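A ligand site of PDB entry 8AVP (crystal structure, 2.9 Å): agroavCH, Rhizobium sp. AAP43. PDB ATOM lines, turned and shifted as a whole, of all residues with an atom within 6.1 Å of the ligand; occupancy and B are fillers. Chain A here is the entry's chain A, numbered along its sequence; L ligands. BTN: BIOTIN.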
ATOM      1  N   ASN A  16     -17.776 -27.035 -10.620  1.00  0.00           N
ATOM      2  CA  ASN A  16     -18.468 -25.834 -11.171  1.00  0.00           C
ATOM      3  C   ASN A  16     -19.918 -26.147 -11.582  1.00  0.00           C
ATOM      4  O   ASN A  16     -20.368 -27.296 -11.407  1.00  0.00           O
ATOM      5  CB  ASN A  16     -17.691 -25.197 -12.328  1.00  0.00           C
ATOM      6  CG  ASN A  16     -17.539 -26.065 -13.552  1.00  0.00           C
ATOM      7  OD1 ASN A  16     -18.173 -27.102 -13.690  1.00  0.00           O
ATOM      8  ND2 ASN A  16     -16.682 -25.633 -14.452  1.00  0.00           N
ATOM      9  N   LEU A  18     -21.453 -26.643 -14.144  1.00  0.00           N
ATOM     10  CA  LEU A  18     -21.601 -27.667 -15.213  1.00  0.00           C
ATOM     11  C   LEU A  18     -21.293 -29.074 -14.646  1.00  0.00           C
ATOM     12  O   LEU A  18     -21.592 -30.071 -15.325  1.00  0.00           O
ATOM     13  CB  LEU A  18     -20.632 -27.301 -16.347  1.00  0.00           C
ATOM     14  CG  LEU A  18     -21.132 -26.334 -17.427  1.00  0.00           C
ATOM     15  CD1 LEU A  18     -22.084 -25.295 -16.909  1.00  0.00           C
ATOM     16  CD2 LEU A  18     -19.971 -25.629 -18.114  1.00  0.00           C
ATOM     17  N   SER A  20     -18.279 -30.217 -13.968  1.00  0.00           N
ATOM     18  CA  SER A  20     -16.848 -30.501 -14.226  1.00  0.00           C
ATOM     19  C   SER A  20     -16.119 -30.508 -12.886  1.00  0.00           C
ATOM     20  O   SER A  20     -16.486 -29.729 -11.997  1.00  0.00           O
ATOM     21  CB  SER A  20     -16.268 -29.501 -15.206  1.00  0.00           C
ATOM     22  OG  SER A  20     -16.950 -29.604 -16.462  1.00  0.00           O
ATOM     23  N   TYR A  36      -8.356 -32.070 -14.482  1.00  0.00           N
ATOM     24  CA  TYR A  36      -9.661 -31.448 -14.829  1.00  0.00           C
ATOM     25  C   TYR A  36     -10.491 -32.534 -15.490  1.00  0.00           C
ATOM     26  O   TYR A  36      -9.987 -33.241 -16.338  1.00  0.00           O
ATOM     27  CB  TYR A  36      -9.496 -30.274 -15.805  1.00  0.00           C
ATOM     28  CG  TYR A  36     -10.649 -29.303 -15.841  1.00  0.00           C
ATOM     29  CD1 TYR A  36     -11.809 -29.587 -16.542  1.00  0.00           C
ATOM     30  CD2 TYR A  36     -10.600 -28.104 -15.155  1.00  0.00           C
ATOM     31  CE1 TYR A  36     -12.870 -28.693 -16.586  1.00  0.00           C
ATOM     32  CE2 TYR A  36     -11.664 -27.208 -15.176  1.00  0.00           C
ATOM     33  CZ  TYR A  36     -12.800 -27.509 -15.888  1.00  0.00           C
ATOM     34  OH  TYR A  36     -13.847 -26.659 -15.878  1.00  0.00           O
ATOM     35  N   VAL A  37     -11.731 -32.696 -15.064  1.00  0.00           N
ATOM     36  CA  VAL A  37     -12.662 -33.677 -15.665  1.00  0.00           C
ATOM     37  C   VAL A  37     -13.839 -32.885 -16.203  1.00  0.00           C
ATOM     38  O   VAL A  37     -14.615 -32.392 -15.360  1.00  0.00           O
ATOM     39  CB  VAL A  37     -13.111 -34.726 -14.638  1.00  0.00           C
ATOM     40  CG1 VAL A  37     -14.029 -35.747 -15.296  1.00  0.00           C
ATOM     41  CG2 VAL A  37     -11.926 -35.402 -13.994  1.00  0.00           C
ATOM     42  N   ASN A  38     -13.947 -32.770 -17.541  1.00  0.00           N
ATOM     43  CA  ASN A  38     -15.022 -31.984 -18.200  1.00  0.00           C
ATOM     44  C   ASN A  38     -16.342 -32.747 -18.081  1.00  0.00           C
ATOM     45  O   ASN A  38     -16.327 -33.975 -18.198  1.00  0.00           O
ATOM     46  CB  ASN A  38     -14.760 -31.721 -19.674  1.00  0.00           C
ATOM     47  CG  ASN A  38     -15.894 -30.928 -20.286  1.00  0.00           C
ATOM     48  OD1 ASN A  38     -16.398 -29.993 -19.671  1.00  0.00           O
ATOM     49  ND2 ASN A  38     -16.316 -31.289 -21.489  1.00  0.00           N
ATOM     50  N   ASN A  39     -17.446 -32.037 -17.863  1.00  0.00           N
ATOM     51  CA  ASN A  39     -18.794 -32.663 -17.805  1.00  0.00           C
ATOM     52  C   ASN A  39     -19.831 -31.777 -18.484  1.00  0.00           C
ATOM     53  O   ASN A  39     -21.031 -31.986 -18.260  1.00  0.00           O
ATOM     54  CB  ASN A  39     -19.260 -32.905 -16.370  1.00  0.00           C
ATOM     55  CG  ASN A  39     -20.619 -33.561 -16.314  1.00  0.00           C
ATOM     56  OD1 ASN A  39     -21.525 -33.060 -15.642  1.00  0.00           O
ATOM     57  ND2 ASN A  39     -20.786 -34.654 -17.029  1.00  0.00           N
ATOM     58  N   ALA A  40     -19.377 -30.820 -19.264  1.00  0.00           N
ATOM     59  CA  ALA A  40     -20.271 -29.797 -19.846  1.00  0.00           C
ATOM     60  C   ALA A  40     -21.092 -30.498 -20.909  1.00  0.00           C
ATOM     61  O   ALA A  40     -20.531 -31.109 -21.817  1.00  0.00           O
ATOM     62  CB  ALA A  40     -19.474 -28.661 -20.433  1.00  0.00           C
ATOM     63  N   GLY A  42     -22.805 -30.999 -24.292  1.00  0.00           N
ATOM     64  CA  GLY A  42     -22.661 -30.464 -25.661  1.00  0.00           C
ATOM     65  C   GLY A  42     -21.237 -30.096 -25.970  1.00  0.00           C
ATOM     66  O   GLY A  42     -21.049 -29.276 -26.852  1.00  0.00           O
ATOM     67  N   THR A  43     -20.280 -30.676 -25.242  1.00  0.00           N
ATOM     68  CA  THR A  43     -18.813 -30.479 -25.409  1.00  0.00           C
ATOM     69  C   THR A  43     -18.222 -31.852 -25.710  1.00  0.00           C
ATOM     70  O   THR A  43     -18.996 -32.824 -25.633  1.00  0.00           O
ATOM     71  CB  THR A  43     -18.173 -29.893 -24.141  1.00  0.00           C
ATOM     72  OG1 THR A  43     -18.420 -30.791 -23.052  1.00  0.00           O
ATOM     73  CG2 THR A  43     -18.679 -28.518 -23.749  1.00  0.00           C
ATOM     74  N   GLY A  44     -16.916 -31.938 -25.980  1.00  0.00           N
ATOM     75  CA  GLY A  44     -16.197 -33.221 -26.115  1.00  0.00           C
ATOM     76  C   GLY A  44     -15.408 -33.553 -24.865  1.00  0.00           C
ATOM     77  O   GLY A  44     -15.346 -32.766 -23.921  1.00  0.00           O
ATOM     78  N   CYS A  45     -14.749 -34.691 -24.858  1.00  0.00           N
ATOM     79  CA  CYS A  45     -13.675 -34.963 -23.880  1.00  0.00           C
ATOM     80  C   CYS A  45     -14.235 -34.970 -22.467  1.00  0.00           C
ATOM     81  O   CYS A  45     -13.614 -34.290 -21.592  1.00  0.00           O
ATOM     82  CB  CYS A  45     -12.612 -33.895 -24.051  1.00  0.00           C
ATOM     83  SG  CYS A  45     -11.641 -34.113 -25.564  1.00  0.00           S
ATOM     84  N   TRP A  67      -6.914 -30.112 -24.463  1.00  0.00           N
ATOM     85  CA  TRP A  67      -7.907 -31.196 -24.436  1.00  0.00           C
ATOM     86  C   TRP A  67      -7.402 -32.381 -25.264  1.00  0.00           C
ATOM     87  O   TRP A  67      -8.057 -32.731 -26.244  1.00  0.00           O
ATOM     88  CB  TRP A  67      -9.249 -30.671 -24.898  1.00  0.00           C
ATOM     89  CG  TRP A  67      -9.838 -29.697 -23.941  1.00  0.00           C
ATOM     90  CD1 TRP A  67     -10.028 -28.374 -24.159  1.00  0.00           C
ATOM     91  CD2 TRP A  67     -10.343 -29.975 -22.622  1.00  0.00           C
ATOM     92  NE1 TRP A  67     -10.610 -27.800 -23.073  1.00  0.00           N
ATOM     93  CE2 TRP A  67     -10.831 -28.755 -22.121  1.00  0.00           C
ATOM     94  CE3 TRP A  67     -10.461 -31.118 -21.842  1.00  0.00           C
ATOM     95  CZ2 TRP A  67     -11.394 -28.637 -20.846  1.00  0.00           C
ATOM     96  CZ3 TRP A  67     -11.021 -31.006 -20.582  1.00  0.00           C
ATOM     97  CH2 TRP A  67     -11.470 -29.786 -20.098  1.00  0.00           C
ATOM     98  N   CYS A  74      -9.805 -33.408 -28.425  1.00  0.00           N
ATOM     99  CA  CYS A  74     -10.828 -32.471 -28.943  1.00  0.00           C
ATOM    100  C   CYS A  74     -10.113 -31.352 -29.698  1.00  0.00           C
ATOM    101  O   CYS A  74     -10.792 -30.545 -30.346  1.00  0.00           O
ATOM    102  CB  CYS A  74     -11.754 -31.955 -27.838  1.00  0.00           C
ATOM    103  SG  CYS A  74     -12.784 -33.254 -27.121  1.00  0.00           S
ATOM    104  N   ARG A  75      -8.778 -31.336 -29.645  1.00  0.00           N
ATOM    105  CA  ARG A  75      -7.933 -30.544 -30.581  1.00  0.00           C
ATOM    106  C   ARG A  75      -8.187 -29.055 -30.313  1.00  0.00           C
ATOM    107  O   ARG A  75      -8.039 -28.186 -31.232  1.00  0.00           O
ATOM    108  CB  ARG A  75      -8.246 -31.086 -31.975  1.00  0.00           C
ATOM    109  CG  ARG A  75      -7.294 -30.575 -33.041  1.00  0.00           C
ATOM    110  CD  ARG A  75      -7.142 -31.530 -34.209  1.00  0.00           C
ATOM    111  NE  ARG A  75      -5.741 -31.624 -34.589  1.00  0.00           N
ATOM    112  CZ  ARG A  75      -4.828 -32.315 -33.913  1.00  0.00           C
ATOM    113  NH1 ARG A  75      -3.582 -32.353 -34.355  1.00  0.00           N
ATOM    114  NH2 ARG A  75      -5.170 -32.962 -32.802  1.00  0.00           N
ATOM    115  N   SER A  76      -8.468 -28.782 -29.043  1.00  0.00           N
ATOM    116  CA  SER A  76      -8.918 -27.504 -28.447  1.00  0.00           C
ATOM    117  C   SER A  76      -8.162 -27.271 -27.133  1.00  0.00           C
ATOM    118  O   SER A  76      -7.630 -28.251 -26.555  1.00  0.00           O
ATOM    119  CB  SER A  76     -10.394 -27.581 -28.193  1.00  0.00           C
ATOM    120  OG  SER A  76     -10.689 -28.602 -27.231  1.00  0.00           O
ATOM    121  N   ALA A  77      -8.153 -26.032 -26.649  1.00  0.00           N
ATOM    122  CA  ALA A  77      -7.435 -25.632 -25.423  1.00  0.00           C
ATOM    123  C   ALA A  77      -8.235 -24.577 -24.655  1.00  0.00           C
ATOM    124  O   ALA A  77      -8.673 -23.578 -25.271  1.00  0.00           O
ATOM    125  CB  ALA A  77      -6.085 -25.089 -25.800  1.00  0.00           C
ATOM    126  N   THR A  78      -8.451 -24.789 -23.366  1.00  0.00           N
ATOM    127  CA  THR A  78      -9.202 -23.830 -22.520  1.00  0.00           C
ATOM    128  C   THR A  78      -8.215 -23.264 -21.519  1.00  0.00           C
ATOM    129  O   THR A  78      -7.410 -24.020 -21.010  1.00  0.00           O
ATOM    130  CB  THR A  78     -10.429 -24.451 -21.814  1.00  0.00           C
ATOM    131  OG1 THR A  78     -11.385 -24.787 -22.823  1.00  0.00           O
ATOM    132  CG2 THR A  78     -11.067 -23.514 -20.802  1.00  0.00           C
ATOM    133  N   TRP A  80      -8.534 -20.615 -17.979  1.00  0.00           N
ATOM    134  CA  TRP A  80      -9.343 -19.856 -17.002  1.00  0.00           C
ATOM    135  C   TRP A  80      -8.446 -18.843 -16.333  1.00  0.00           C
ATOM    136  O   TRP A  80      -7.276 -19.162 -16.136  1.00  0.00           O
ATOM    137  CB  TRP A  80      -9.965 -20.734 -15.904  1.00  0.00           C
ATOM    138  CG  TRP A  80     -10.911 -21.796 -16.364  1.00  0.00           C
ATOM    139  CD1 TRP A  80     -12.268 -21.831 -16.196  1.00  0.00           C
ATOM    140  CD2 TRP A  80     -10.553 -23.025 -17.022  1.00  0.00           C
ATOM    141  NE1 TRP A  80     -12.780 -22.992 -16.714  1.00  0.00           N
ATOM    142  CE2 TRP A  80     -11.747 -23.745 -17.207  1.00  0.00           C
ATOM    143  CE3 TRP A  80      -9.350 -23.581 -17.470  1.00  0.00           C
ATOM    144  CZ2 TRP A  80     -11.765 -24.997 -17.811  1.00  0.00           C
ATOM    145  CZ3 TRP A  80      -9.359 -24.798 -18.080  1.00  0.00           C
ATOM    146  CH2 TRP A  80     -10.548 -25.500 -18.233  1.00  0.00           C
ATOM    147  N   TRP A  98     -13.366 -17.973 -18.805  1.00  0.00           N
ATOM    148  CA  TRP A  98     -12.657 -18.983 -19.627  1.00  0.00           C
ATOM    149  C   TRP A  98     -12.734 -18.637 -21.110  1.00  0.00           C
ATOM    150  O   TRP A  98     -13.611 -17.943 -21.539  1.00  0.00           O
ATOM    151  CB  TRP A  98     -13.162 -20.394 -19.321  1.00  0.00           C
ATOM    152  CG  TRP A  98     -14.597 -20.695 -19.591  1.00  0.00           C
ATOM    153  CD1 TRP A  98     -15.604 -20.835 -18.673  1.00  0.00           C
ATOM    154  CD2 TRP A  98     -15.189 -20.997 -20.874  1.00  0.00           C
ATOM    155  NE1 TRP A  98     -16.777 -21.153 -19.310  1.00  0.00           N
ATOM    156  CE2 TRP A  98     -16.554 -21.270 -20.649  1.00  0.00           C
ATOM    157  CE3 TRP A  98     -14.691 -21.045 -22.182  1.00  0.00           C
ATOM    158  CZ2 TRP A  98     -17.428 -21.559 -21.690  1.00  0.00           C
ATOM    159  CZ3 TRP A  98     -15.564 -21.338 -23.214  1.00  0.00           C
ATOM    160  CH2 TRP A  98     -16.905 -21.599 -22.963  1.00  0.00           C
ATOM    161  N   LEU A 100     -12.023 -20.946 -24.676  1.00  0.00           N
ATOM    162  CA  LEU A 100     -11.807 -22.287 -25.281  1.00  0.00           C
ATOM    163  C   LEU A 100     -11.536 -22.027 -26.758  1.00  0.00           C
ATOM    164  O   LEU A 100     -12.424 -21.463 -27.391  1.00  0.00           O
ATOM    165  CB  LEU A 100     -13.077 -23.128 -25.097  1.00  0.00           C
ATOM    166  CG  LEU A 100     -13.251 -24.293 -26.067  1.00  0.00           C
ATOM    167  CD1 LEU A 100     -11.972 -25.092 -26.197  1.00  0.00           C
ATOM    168  CD2 LEU A 100     -14.346 -25.233 -25.618  1.00  0.00           C
ATOM    169  N   PHE A 102     -10.486 -23.603 -30.578  1.00  0.00           N
ATOM    170  CA  PHE A 102     -10.505 -24.885 -31.324  1.00  0.00           C
ATOM    171  C   PHE A 102     -10.476 -24.625 -32.834  1.00  0.00           C
ATOM    172  O   PHE A 102     -10.783 -23.493 -33.249  1.00  0.00           O
ATOM    173  CB  PHE A 102     -11.728 -25.718 -30.971  1.00  0.00           C
ATOM    174  CG  PHE A 102     -13.045 -25.054 -31.294  1.00  0.00           C
ATOM    175  CD1 PHE A 102     -13.560 -24.072 -30.458  1.00  0.00           C
ATOM    176  CD2 PHE A 102     -13.772 -25.431 -32.403  1.00  0.00           C
ATOM    177  CE1 PHE A 102     -14.777 -23.466 -30.758  1.00  0.00           C
ATOM    178  CE2 PHE A 102     -14.978 -24.815 -32.711  1.00  0.00           C
ATOM    179  CZ  PHE A 102     -15.475 -23.839 -31.881  1.00  0.00           C
ATOM    180  N   ASN A 115     -17.497 -19.325 -15.210  1.00  0.00           N
ATOM    181  CA  ASN A 115     -17.504 -20.650 -14.543  1.00  0.00           C
ATOM    182  C   ASN A 115     -17.278 -20.382 -13.064  1.00  0.00           C
ATOM    183  O   ASN A 115     -16.269 -19.696 -12.767  1.00  0.00           O
ATOM    184  CB  ASN A 115     -16.354 -21.547 -15.004  1.00  0.00           C
ATOM    185  CG  ASN A 115     -16.754 -22.671 -15.930  1.00  0.00           C
ATOM    186  OD1 ASN A 115     -16.008 -23.636 -16.105  1.00  0.00           O
ATOM    187  ND2 ASN A 115     -17.921 -22.534 -16.543  1.00  0.00           N
ATOM    188  N   PHE A 117     -16.327 -22.238  -9.531  1.00  0.00           N
ATOM    189  CA  PHE A 117     -15.843 -23.501  -8.913  1.00  0.00           C
ATOM    190  C   PHE A 117     -15.990 -23.394  -7.397  1.00  0.00           C
ATOM    191  O   PHE A 117     -15.518 -22.388  -6.840  1.00  0.00           O
ATOM    192  CB  PHE A 117     -14.374 -23.780  -9.196  1.00  0.00           C
ATOM    193  CG  PHE A 117     -14.060 -23.970 -10.655  1.00  0.00           C
ATOM    194  CD1 PHE A 117     -14.096 -25.223 -11.211  1.00  0.00           C
ATOM    195  CD2 PHE A 117     -13.770 -22.887 -11.458  1.00  0.00           C
ATOM    196  CE1 PHE A 117     -13.841 -25.403 -12.554  1.00  0.00           C
ATOM    197  CE2 PHE A 117     -13.533 -23.056 -12.803  1.00  0.00           C
ATOM    198  CZ  PHE A 117     -13.572 -24.327 -13.346  1.00  0.00           C
HETATM  199  C11 BTN L   1     -13.901 -29.271 -26.478  1.00  0.00           C
HETATM  200  O11 BTN L   1     -15.024 -28.782 -26.465  1.00  0.00           O
HETATM  201  O12 BTN L   1     -13.158 -29.221 -27.473  1.00  0.00           O
HETATM  202  C10 BTN L   1     -13.378 -29.950 -25.213  1.00  0.00           C
HETATM  203  C9  BTN L   1     -14.234 -29.778 -23.981  1.00  0.00           C
HETATM  204  C8  BTN L   1     -14.235 -28.361 -23.401  1.00  0.00           C
HETATM  205  C7  BTN L   1     -14.968 -28.153 -22.065  1.00  0.00           C
HETATM  206  C2  BTN L   1     -15.399 -26.726 -21.736  1.00  0.00           C
HETATM  207  S1  BTN L   1     -13.951 -25.793 -21.156  1.00  0.00           S
HETATM  208  C6  BTN L   1     -15.150 -24.458 -20.889  1.00  0.00           C
HETATM  209  C5  BTN L   1     -16.300 -25.076 -20.090  1.00  0.00           C
HETATM  210  N1  BTN L   1     -15.994 -25.274 -18.699  1.00  0.00           N
HETATM  211  C3  BTN L   1     -16.127 -26.561 -18.324  1.00  0.00           C
HETATM  212  O3  BTN L   1     -16.066 -26.984 -17.153  1.00  0.00           O
HETATM  213  N2  BTN L   1     -16.313 -27.330 -19.435  1.00  0.00           N
HETATM  214  C4  BTN L   1     -16.468 -26.535 -20.635  1.00  0.00           C
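The side-chain hydroxyl of Ser 20 sits at hydrogen-bond distance from an oxygen (O3) of the ligand (2.9 Å). A nitrogen (N1) of the ligand lies within hydrogen-bond range of the side-chain amide oxygen (OD1) of Asn 115. OG of Ser 76 is in hydrogen-bond range of O12 of the ligand (2.6 Å). O3 of the ligand lies within hydrogen-bond range of ND2 of Asn 16, at 3.1 Å. The side-chain hydroxyl (OH) of Tyr 36 is in hydrogen-bond range of an oxygen (O3) of the ligand (2.6 Å). OG1 of Thr 78 sits close to S1 of the ligand, 3.2 Å away. The side-chain amide oxygen (OD1) of Asn 38 sits at hydrogen-bond distance from a nitrogen (N2) of the ligand (2.7 Å).
The indole nitrogen of Trp 67 sits at hydrogen-bond distance from the side-chain hydroxyl of Thr 78 (3.1 Å). O of Leu 18 sits close to OD1 of Asn 39 (3.0 Å). OD1 of Asn 16 sits at hydrogen-bond distance from N of Ser 20 (3.1 Å). N of Cys 74 is in hydrogen-bond range of O of Trp 67, 2.9 Å away. OD1 of Asn 38 is in hydrogen-bond range of OG of Ser 20, at 3.3 Å. OD1 of Asn 115 is in hydrogen-bond range of NE1 of Trp 80 (3.3 Å). The side-chain hydroxyl (OH) of Tyr 36 lies within hydrogen-bond range of the side-chain amide nitrogen (ND2) of Asn 16 (3.3 Å). The backbone carbonyl oxygen (O) of Ala 40 is in hydrogen-bond range of the side-chain hydroxyl (OG1) of Thr 43, 2.5 Å away.
Leu 18 touches the ligand (CD2 to C3, 3.96 Å). Ala 40 touches the ligand (CB to N2, 3.6 Å). CB of Thr 43 touches C9 of the ligand, at 3.9 Å. Gly 44 touches the ligand. CE2 of Trp 67 touches C8 of the ligand (3.7 Å). CB of Cys 74 touches O12 of the ligand, at 3.1 Å. Trp 98 touches the ligand (CD2 to C6, 3.5 Å). Leu 100 touches the ligand. 15 residues have an atom within 4 Å of the ligand: Asn 16, Leu 18, Ser 20, Tyr 36, Asn 38, Ala 40, Thr 43, Gly 44, Trp 67, Cys 74, Ser 76, Thr 78, Trp 98, Leu 100 and Asn 115. The nearest printed residue that does not touch the ligand is Trp 80 (4.1 Å).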
